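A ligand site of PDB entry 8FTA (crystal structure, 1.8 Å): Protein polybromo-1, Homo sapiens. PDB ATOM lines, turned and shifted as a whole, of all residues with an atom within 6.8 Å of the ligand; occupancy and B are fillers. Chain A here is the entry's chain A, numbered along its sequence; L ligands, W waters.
Leu 32 touches the ligand (O to C13, 3.2 Å).
O of Phe 33 touches C12 of the ligand, at 3.6 Å.
Lys 35 touches the ligand (O to C13, 3.3 Å).
CA of Leu 36 touches C13 of the ligand (3.9 Å).
Pro 37 touches the ligand (CG to N1, 3.7 Å).
Tyr 42 touches the ligand (CD1 to C7, 3.6 Å).
Ile 53 touches the ligand.
Asp 54 touches the ligand (CB to C12, 3.9 Å).
Leu 80 touches the ligand (O to CL1, 3.1 Å).
Asn 83 touches the ligand.
Tyr 87 touches the ligand.
Val 94 touches the ligand.
Hydrophobic or aromatic side chains within 4 Å of the ligand: Phe 33, Pro 37, Tyr 42, Tyr 45, Leu 80, Ala 84, Tyr 87 and Val 94.
15 residues have an atom within 4 Å of the ligand: Leu 32, Phe 33, Lys 35, Leu 36, Pro 37, Tyr 42, Tyr 45, Ile 53, Asp 54, Leu 80, Asn 83, Ala 84, Tyr 87, Asn 88 and Val 94.
The nearest printed residue that does not touch the ligand is Gln 34 (4.7 Å).
Water W2 lies within hydrogen-bond range of OH of Tyr 45 (2.7 Å), O of Ile 53 (2.8 Å) and ND2 of Asn 83 (2.9 Å).
The side-chain hydroxyl (OH) of Tyr 45 sits at hydrogen-bond distance from an oxygen (O1) of the ligand, 2.9 Å away.
The side-chain amide oxygen (OD1) of Asn 88 lies within hydrogen-bond range of a nitrogen (N2) of the ligand (3.0 Å).
The backbone NH (N) of Ala 84 sits close to an oxygen (O1) of the ligand (3.5 Å).
The side-chain amide oxygen (OD1) of Asn 88 sits close to the backbone carbonyl oxygen (O) of Ala 84 (3.4 Å).
N of Leu 55 lies within hydrogen-bond range of O of Phe 33.
The backbone NH of Leu 36 sits at hydrogen-bond distance from the side-chain carboxylate of Asp 54 (2.9 Å).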
ATOM      1  N   LEU A  32      17.462  -9.728 -10.636  1.00  0.00           N
ATOM      2  CA  LEU A  32      16.356  -9.601 -11.575  1.00  0.00           C
ATOM      3  C   LEU A  32      15.022 -10.035 -10.995  1.00  0.00           C
ATOM      4  O   LEU A  32      14.006  -9.996 -11.710  1.00  0.00           O
ATOM      5  CB  LEU A  32      16.672 -10.428 -12.828  1.00  0.00           C
ATOM      6  CG  LEU A  32      17.868  -9.865 -13.625  1.00  0.00           C
ATOM      7  CD1 LEU A  32      17.919 -10.423 -15.022  1.00  0.00           C
ATOM      8  CD2 LEU A  32      17.765  -8.342 -13.679  1.00  0.00           C
ATOM      9  N   PHE A  33      14.974 -10.434  -9.728  1.00  0.00           N
ATOM     10  CA  PHE A  33      13.743 -10.912  -9.110  1.00  0.00           C
ATOM     11  C   PHE A  33      13.218  -9.983  -8.038  1.00  0.00           C
ATOM     12  O   PHE A  33      12.193 -10.297  -7.412  1.00  0.00           O
ATOM     13  CB  PHE A  33      13.964 -12.302  -8.499  1.00  0.00           C
ATOM     14  CG  PHE A  33      14.366 -13.353  -9.486  1.00  0.00           C
ATOM     15  CD1 PHE A  33      15.676 -13.467  -9.907  1.00  0.00           C
ATOM     16  CD2 PHE A  33      13.430 -14.244  -9.978  1.00  0.00           C
ATOM     17  CE1 PHE A  33      16.040 -14.431 -10.817  1.00  0.00           C
ATOM     18  CE2 PHE A  33      13.789 -15.224 -10.882  1.00  0.00           C
ATOM     19  CZ  PHE A  33      15.100 -15.309 -11.308  1.00  0.00           C
ATOM     20  N   GLN A  34      13.903  -8.865  -7.781  1.00  0.00           N
ATOM     21  CA  GLN A  34      13.454  -7.945  -6.735  1.00  0.00           C
ATOM     22  C   GLN A  34      12.097  -7.336  -7.090  1.00  0.00           C
ATOM     23  O   GLN A  34      11.200  -7.264  -6.241  1.00  0.00           O
ATOM     24  CB  GLN A  34      14.497  -6.849  -6.531  1.00  0.00           C
ATOM     25  CG  GLN A  34      15.707  -7.291  -5.734  1.00  0.00           C
ATOM     26  CD  GLN A  34      15.415  -7.479  -4.255  1.00  0.00           C
ATOM     27  OE1 GLN A  34      14.321  -7.187  -3.781  1.00  0.00           O
ATOM     28  NE2 GLN A  34      16.422  -7.950  -3.524  1.00  0.00           N
ATOM     29  N   LYS A  35      11.930  -6.893  -8.337  1.00  0.00           N
ATOM     30  CA  LYS A  35      10.783  -6.086  -8.729  1.00  0.00           C
ATOM     31  C   LYS A  35      10.160  -6.667  -9.993  1.00  0.00           C
ATOM     32  O   LYS A  35      10.876  -6.947 -10.959  1.00  0.00           O
ATOM     33  CB  LYS A  35      11.228  -4.640  -8.966  1.00  0.00           C
ATOM     34  CG  LYS A  35      10.097  -3.681  -9.290  1.00  0.00           C
ATOM     35  CD  LYS A  35       9.125  -3.599  -8.123  1.00  0.00           C
ATOM     36  CE  LYS A  35       7.712  -3.257  -8.582  1.00  0.00           C
ATOM     37  NZ  LYS A  35       6.919  -2.648  -7.471  1.00  0.00           N
ATOM     38  N   LEU A  36       8.845  -6.853  -9.969  1.00  0.00           N
ATOM     39  CA  LEU A  36       8.151  -7.392 -11.130  1.00  0.00           C
ATOM     40  C   LEU A  36       8.346  -6.475 -12.338  1.00  0.00           C
ATOM     41  O   LEU A  36       8.535  -5.255 -12.184  1.00  0.00           O
ATOM     42  CB  LEU A  36       6.658  -7.516 -10.838  1.00  0.00           C
ATOM     43  CG  LEU A  36       6.154  -8.758 -10.080  1.00  0.00           C
ATOM     44  CD1 LEU A  36       4.739  -8.511  -9.624  1.00  0.00           C
ATOM     45  CD2 LEU A  36       6.216  -9.960 -10.990  1.00  0.00           C
ATOM     46  N   PRO A  37       8.269  -7.018 -13.552  1.00  0.00           N
ATOM     47  CA  PRO A  37       8.351  -6.178 -14.757  1.00  0.00           C
ATOM     48  C   PRO A  37       7.189  -5.199 -14.850  1.00  0.00           C
ATOM     49  O   PRO A  37       6.072  -5.471 -14.404  1.00  0.00           O
ATOM     50  CB  PRO A  37       8.313  -7.190 -15.914  1.00  0.00           C
ATOM     51  CG  PRO A  37       8.416  -8.539 -15.329  1.00  0.00           C
ATOM     52  CD  PRO A  37       8.058  -8.444 -13.859  1.00  0.00           C
ATOM     53  N   TYR A  42       6.050  -4.656 -20.321  1.00  0.00           N
ATOM     54  CA  TYR A  42       5.996  -6.109 -20.449  1.00  0.00           C
ATOM     55  C   TYR A  42       4.571  -6.606 -20.205  1.00  0.00           C
ATOM     56  O   TYR A  42       4.296  -7.356 -19.259  1.00  0.00           O
ATOM     57  CB  TYR A  42       7.006  -6.762 -19.499  1.00  0.00           C
ATOM     58  CG  TYR A  42       8.358  -6.284 -19.921  1.00  0.00           C
ATOM     59  CD1 TYR A  42       9.030  -6.903 -20.973  1.00  0.00           C
ATOM     60  CD2 TYR A  42       8.947  -5.153 -19.339  1.00  0.00           C
ATOM     61  CE1 TYR A  42      10.223  -6.446 -21.425  1.00  0.00           C
ATOM     62  CE2 TYR A  42      10.143  -4.688 -19.785  1.00  0.00           C
ATOM     63  CZ  TYR A  42      10.781  -5.323 -20.833  1.00  0.00           C
ATOM     64  OH  TYR A  42      11.991  -4.862 -21.281  1.00  0.00           O
ATOM     65  N   TYR A  45       3.794 -10.421 -19.897  1.00  0.00           N
ATOM     66  CA  TYR A  45       4.067 -11.087 -18.637  1.00  0.00           C
ATOM     67  C   TYR A  45       2.790 -11.319 -17.851  1.00  0.00           C
ATOM     68  O   TYR A  45       2.592 -12.391 -17.248  1.00  0.00           O
ATOM     69  CB  TYR A  45       5.063 -10.264 -17.811  1.00  0.00           C
ATOM     70  CG  TYR A  45       5.598 -11.024 -16.615  1.00  0.00           C
ATOM     71  CD1 TYR A  45       4.935 -10.997 -15.398  1.00  0.00           C
ATOM     72  CD2 TYR A  45       6.739 -11.811 -16.726  1.00  0.00           C
ATOM     73  CE1 TYR A  45       5.424 -11.717 -14.299  1.00  0.00           C
ATOM     74  CE2 TYR A  45       7.243 -12.527 -15.640  1.00  0.00           C
ATOM     75  CZ  TYR A  45       6.568 -12.479 -14.445  1.00  0.00           C
ATOM     76  OH  TYR A  45       7.039 -13.202 -13.367  1.00  0.00           O
ATOM     77  N   ILE A  49       1.462 -14.951 -16.809  1.00  0.00           N
ATOM     78  CA  ILE A  49       1.706 -15.298 -15.416  1.00  0.00           C
ATOM     79  C   ILE A  49       0.474 -14.939 -14.597  1.00  0.00           C
ATOM     80  O   ILE A  49       0.164 -13.757 -14.428  1.00  0.00           O
ATOM     81  CB  ILE A  49       2.947 -14.580 -14.873  1.00  0.00           C
ATOM     82  CG1 ILE A  49       4.197 -15.018 -15.650  1.00  0.00           C
ATOM     83  CG2 ILE A  49       3.075 -14.817 -13.357  1.00  0.00           C
ATOM     84  CD1 ILE A  49       4.453 -16.530 -15.653  1.00  0.00           C
ATOM     85  N   ILE A  53       4.645 -12.358  -8.662  1.00  0.00           N
ATOM     86  CA  ILE A  53       5.252 -12.148  -7.355  1.00  0.00           C
ATOM     87  C   ILE A  53       6.718 -11.761  -7.544  1.00  0.00           C
ATOM     88  O   ILE A  53       7.364 -12.144  -8.530  1.00  0.00           O
ATOM     89  CB  ILE A  53       5.085 -13.407  -6.473  1.00  0.00           C
ATOM     90  CG1 ILE A  53       5.417 -13.091  -5.007  1.00  0.00           C
ATOM     91  CG2 ILE A  53       5.961 -14.562  -7.001  1.00  0.00           C
ATOM     92  CD1 ILE A  53       5.179 -14.291  -4.062  1.00  0.00           C
ATOM     93  N   ASP A  54       7.257 -11.004  -6.589  1.00  0.00           N
ATOM     94  CA  ASP A  54       8.665 -10.636  -6.604  1.00  0.00           C
ATOM     95  C   ASP A  54       9.202 -10.684  -5.183  1.00  0.00           C
ATOM     96  O   ASP A  54       8.453 -10.862  -4.223  1.00  0.00           O
ATOM     97  CB  ASP A  54       8.887  -9.243  -7.242  1.00  0.00           C
ATOM     98  CG  ASP A  54       8.017  -8.158  -6.624  1.00  0.00           C
ATOM     99  OD1 ASP A  54       7.637  -8.287  -5.452  1.00  0.00           O
ATOM    100  OD2 ASP A  54       7.739  -7.135  -7.297  1.00  0.00           O
ATOM    101  N   LEU A  55      10.508 -10.474  -5.043  1.00  0.00           N
ATOM    102  CA  LEU A  55      11.092 -10.527  -3.710  1.00  0.00           C
ATOM    103  C   LEU A  55      10.663  -9.334  -2.858  1.00  0.00           C
ATOM    104  O   LEU A  55      10.571  -9.464  -1.626  1.00  0.00           O
ATOM    105  CB  LEU A  55      12.622 -10.600  -3.781  1.00  0.00           C
ATOM    106  CG  LEU A  55      13.168 -11.916  -4.361  1.00  0.00           C
ATOM    107  CD1 LEU A  55      14.671 -11.800  -4.613  1.00  0.00           C
ATOM    108  CD2 LEU A  55      12.878 -13.104  -3.439  1.00  0.00           C
ATOM    109  N   LEU A  79       6.556 -20.266  -6.211  1.00  0.00           N
ATOM    110  CA  LEU A  79       5.813 -19.552  -7.241  1.00  0.00           C
ATOM    111  C   LEU A  79       6.718 -18.608  -8.005  1.00  0.00           C
ATOM    112  O   LEU A  79       6.642 -18.517  -9.237  1.00  0.00           O
ATOM    113  CB  LEU A  79       4.662 -18.776  -6.593  1.00  0.00           C
ATOM    114  CG  LEU A  79       3.729 -17.964  -7.481  1.00  0.00           C
ATOM    115  CD1 LEU A  79       3.008 -18.901  -8.453  1.00  0.00           C
ATOM    116  CD2 LEU A  79       2.736 -17.225  -6.609  1.00  0.00           C
ATOM    117  N   LEU A  80       7.564 -17.872  -7.283  1.00  0.00           N
ATOM    118  CA  LEU A  80       8.545 -16.999  -7.925  1.00  0.00           C
ATOM    119  C   LEU A  80       9.341 -17.750  -8.973  1.00  0.00           C
ATOM    120  O   LEU A  80       9.450 -17.315 -10.129  1.00  0.00           O
ATOM    121  CB  LEU A  80       9.472 -16.405  -6.869  1.00  0.00           C
ATOM    122  CG  LEU A  80      10.518 -15.358  -7.290  1.00  0.00           C
ATOM    123  CD1 LEU A  80       9.928 -13.959  -7.313  1.00  0.00           C
ATOM    124  CD2 LEU A  80      11.714 -15.415  -6.335  1.00  0.00           C
ATOM    125  N   ALA A  81       9.889 -18.915  -8.598  1.00  0.00           N
ATOM    126  CA  ALA A  81      10.695 -19.679  -9.532  1.00  0.00           C
ATOM    127  C   ALA A  81       9.843 -20.234 -10.676  1.00  0.00           C
ATOM    128  O   ALA A  81      10.271 -20.226 -11.835  1.00  0.00           O
ATOM    129  CB  ALA A  81      11.416 -20.813  -8.803  1.00  0.00           C
ATOM    130  N   LYS A  82       8.643 -20.727 -10.364  1.00  0.00           N
ATOM    131  CA  LYS A  82       7.802 -21.317 -11.400  1.00  0.00           C
ATOM    132  C   LYS A  82       7.433 -20.267 -12.440  1.00  0.00           C
ATOM    133  O   LYS A  82       7.423 -20.541 -13.643  1.00  0.00           O
ATOM    134  CB  LYS A  82       6.553 -21.930 -10.786  1.00  0.00           C
ATOM    135  CG  LYS A  82       5.475 -22.322 -11.804  1.00  0.00           C
ATOM    136  CD  LYS A  82       4.254 -22.919 -11.122  1.00  0.00           C
ATOM    137  CE  LYS A  82       3.362 -23.638 -12.135  1.00  0.00           C
ATOM    138  NZ  LYS A  82       2.151 -24.259 -11.496  1.00  0.00           N
ATOM    139  N   ASN A  83       7.171 -19.042 -11.989  1.00  0.00           N
ATOM    140  CA  ASN A  83       6.804 -17.977 -12.930  1.00  0.00           C
ATOM    141  C   ASN A  83       7.970 -17.660 -13.856  1.00  0.00           C
ATOM    142  O   ASN A  83       7.780 -17.509 -15.073  1.00  0.00           O
ATOM    143  CB  ASN A  83       6.373 -16.727 -12.169  1.00  0.00           C
ATOM    144  CG  ASN A  83       5.024 -16.881 -11.482  1.00  0.00           C
ATOM    145  OD1 ASN A  83       4.275 -17.839 -11.742  1.00  0.00           O
ATOM    146  ND2 ASN A  83       4.703 -15.934 -10.607  1.00  0.00           N
ATOM    147  N   ALA A  84       9.181 -17.546 -13.302  1.00  0.00           N
ATOM    148  CA  ALA A  84      10.349 -17.264 -14.131  1.00  0.00           C
ATOM    149  C   ALA A  84      10.622 -18.405 -15.109  1.00  0.00           C
ATOM    150  O   ALA A  84      11.009 -18.167 -16.253  1.00  0.00           O
ATOM    151  CB  ALA A  84      11.579 -17.031 -13.242  1.00  0.00           C
ATOM    152  N   LYS A  85      10.408 -19.637 -14.668  1.00  0.00           N
ATOM    153  CA  LYS A  85      10.626 -20.783 -15.540  1.00  0.00           C
ATOM    154  C   LYS A  85       9.479 -20.988 -16.542  1.00  0.00           C
ATOM    155  O   LYS A  85       9.630 -21.782 -17.478  1.00  0.00           O
ATOM    156  CB  LYS A  85      10.843 -22.037 -14.690  1.00  0.00           C
ATOM    157  CG  LYS A  85      12.167 -21.951 -13.882  1.00  0.00           C
ATOM    158  CD  LYS A  85      12.215 -22.886 -12.655  1.00  0.00           C
ATOM    159  CE  LYS A  85      12.056 -24.343 -13.068  1.00  0.00           C
ATOM    160  NZ  LYS A  85      12.139 -25.233 -11.849  1.00  0.00           N
ATOM    161  N   THR A  86       8.359 -20.280 -16.372  1.00  0.00           N
ATOM    162  CA  THR A  86       7.289 -20.257 -17.367  1.00  0.00           C
ATOM    163  C   THR A  86       7.495 -19.153 -18.394  1.00  0.00           C
ATOM    164  O   THR A  86       7.328 -19.376 -19.600  1.00  0.00           O
ATOM    165  CB  THR A  86       5.931 -20.072 -16.670  1.00  0.00           C
ATOM    166  OG1 THR A  86       5.713 -21.150 -15.739  1.00  0.00           O
ATOM    167  CG2 THR A  86       4.778 -20.002 -17.665  1.00  0.00           C
ATOM    168  N   TYR A  87       7.890 -17.972 -17.932  1.00  0.00           N
ATOM    169  CA  TYR A  87       7.966 -16.813 -18.826  1.00  0.00           C
ATOM    170  C   TYR A  87       9.270 -16.794 -19.607  1.00  0.00           C
ATOM    171  O   TYR A  87       9.271 -16.505 -20.809  1.00  0.00           O
ATOM    172  CB  TYR A  87       7.836 -15.517 -18.021  1.00  0.00           C
ATOM    173  CG  TYR A  87       7.852 -14.286 -18.910  1.00  0.00           C
ATOM    174  CD1 TYR A  87       6.683 -13.841 -19.509  1.00  0.00           C
ATOM    175  CD2 TYR A  87       9.020 -13.567 -19.121  1.00  0.00           C
ATOM    176  CE1 TYR A  87       6.672 -12.708 -20.324  1.00  0.00           C
ATOM    177  CE2 TYR A  87       9.030 -12.436 -19.945  1.00  0.00           C
ATOM    178  CZ  TYR A  87       7.846 -12.017 -20.536  1.00  0.00           C
ATOM    179  OH  TYR A  87       7.823 -10.902 -21.339  1.00  0.00           O
ATOM    180  N   ASN A  88      10.375 -17.106 -18.943  1.00  0.00           N
ATOM    181  CA  ASN A  88      11.698 -17.031 -19.531  1.00  0.00           C
ATOM    182  C   ASN A  88      12.111 -18.397 -20.046  1.00  0.00           C
ATOM    183  O   ASN A  88      11.665 -19.432 -19.553  1.00  0.00           O
ATOM    184  CB  ASN A  88      12.704 -16.481 -18.510  1.00  0.00           C
ATOM    185  CG  ASN A  88      12.333 -15.101 -18.052  1.00  0.00           C
ATOM    186  OD1 ASN A  88      11.567 -14.925 -17.114  1.00  0.00           O
ATOM    187  ND2 ASN A  88      12.832 -14.097 -18.756  1.00  0.00           N
ATOM    188  N   VAL A  94      18.028 -16.198 -16.384  1.00  0.00           N
ATOM    189  CA  VAL A  94      16.935 -15.984 -15.431  1.00  0.00           C
ATOM    190  C   VAL A  94      16.342 -17.311 -14.998  1.00  0.00           C
ATOM    191  O   VAL A  94      16.056 -17.528 -13.812  1.00  0.00           O
ATOM    192  CB  VAL A  94      15.870 -15.054 -16.042  1.00  0.00           C
ATOM    193  CG1 VAL A  94      14.731 -14.831 -15.060  1.00  0.00           C
ATOM    194  CG2 VAL A  94      16.493 -13.724 -16.426  1.00  0.00           C
ATOM    195  N   ALA A  98      16.535 -18.658 -11.177  1.00  0.00           N
ATOM    196  CA  ALA A  98      15.311 -19.011 -10.449  1.00  0.00           C
ATOM    197  C   ALA A  98      15.496 -20.331  -9.703  1.00  0.00           C
ATOM    198  O   ALA A  98      15.170 -20.434  -8.507  1.00  0.00           O
ATOM    199  CB  ALA A  98      14.129 -19.104 -11.407  1.00  0.00           C
HETATM  200  C1  LIG L   1      13.020 -10.194 -18.755  1.00  0.00           C
HETATM  201  C2  LIG L   1      11.343 -10.555 -17.064  1.00  0.00           C
HETATM  202  C3  LIG L   1      10.430 -13.188 -13.855  1.00  0.00           C
HETATM  203  C4  LIG L   1      10.833 -11.013 -12.903  1.00  0.00           C
HETATM  204  C5  LIG L   1      10.445 -12.347 -12.720  1.00  0.00           C
HETATM  205  C6  LIG L   1      11.709 -10.088 -18.323  1.00  0.00           C
HETATM  206  C7  LIG L   1      10.763  -9.503 -19.132  1.00  0.00           C
HETATM  207  C8  LIG L   1      11.984 -11.616 -14.962  1.00  0.00           C
HETATM  208  C9  LIG L   1      12.305 -11.145 -16.239  1.00  0.00           C
HETATM  209  C10 LIG L   1      10.041 -12.752 -11.436  1.00  0.00           C
HETATM  210  C11 LIG L   1      10.041 -11.860 -10.361  1.00  0.00           C
HETATM  211  C12 LIG L   1      10.437 -10.544 -10.557  1.00  0.00           C
HETATM  212  C13 LIG L   1      10.833 -10.121 -11.828  1.00  0.00           C
HETATM  213  C14 LIG L   1      13.624 -11.240 -16.689  1.00  0.00           C
HETATM  214  C15 LIG L   1      13.976 -10.770 -17.947  1.00  0.00           C
HETATM  215  N1  LIG L   1      11.252 -10.592 -14.164  1.00  0.00           N
HETATM  216  N2  LIG L   1      11.163 -12.841 -14.993  1.00  0.00           N
HETATM  217  O1  LIG L   1       9.673 -14.154 -13.929  1.00  0.00           O
HETATM  218 CL1  LIG L   1       9.568 -14.387 -11.095  1.00  0.00          CL
HETATM  219  O   HOH W   1       9.956 -10.298 -22.293  1.00  0.00           O
HETATM  220  O   HOH W   2       6.375 -13.530 -10.742  1.00  0.00           O
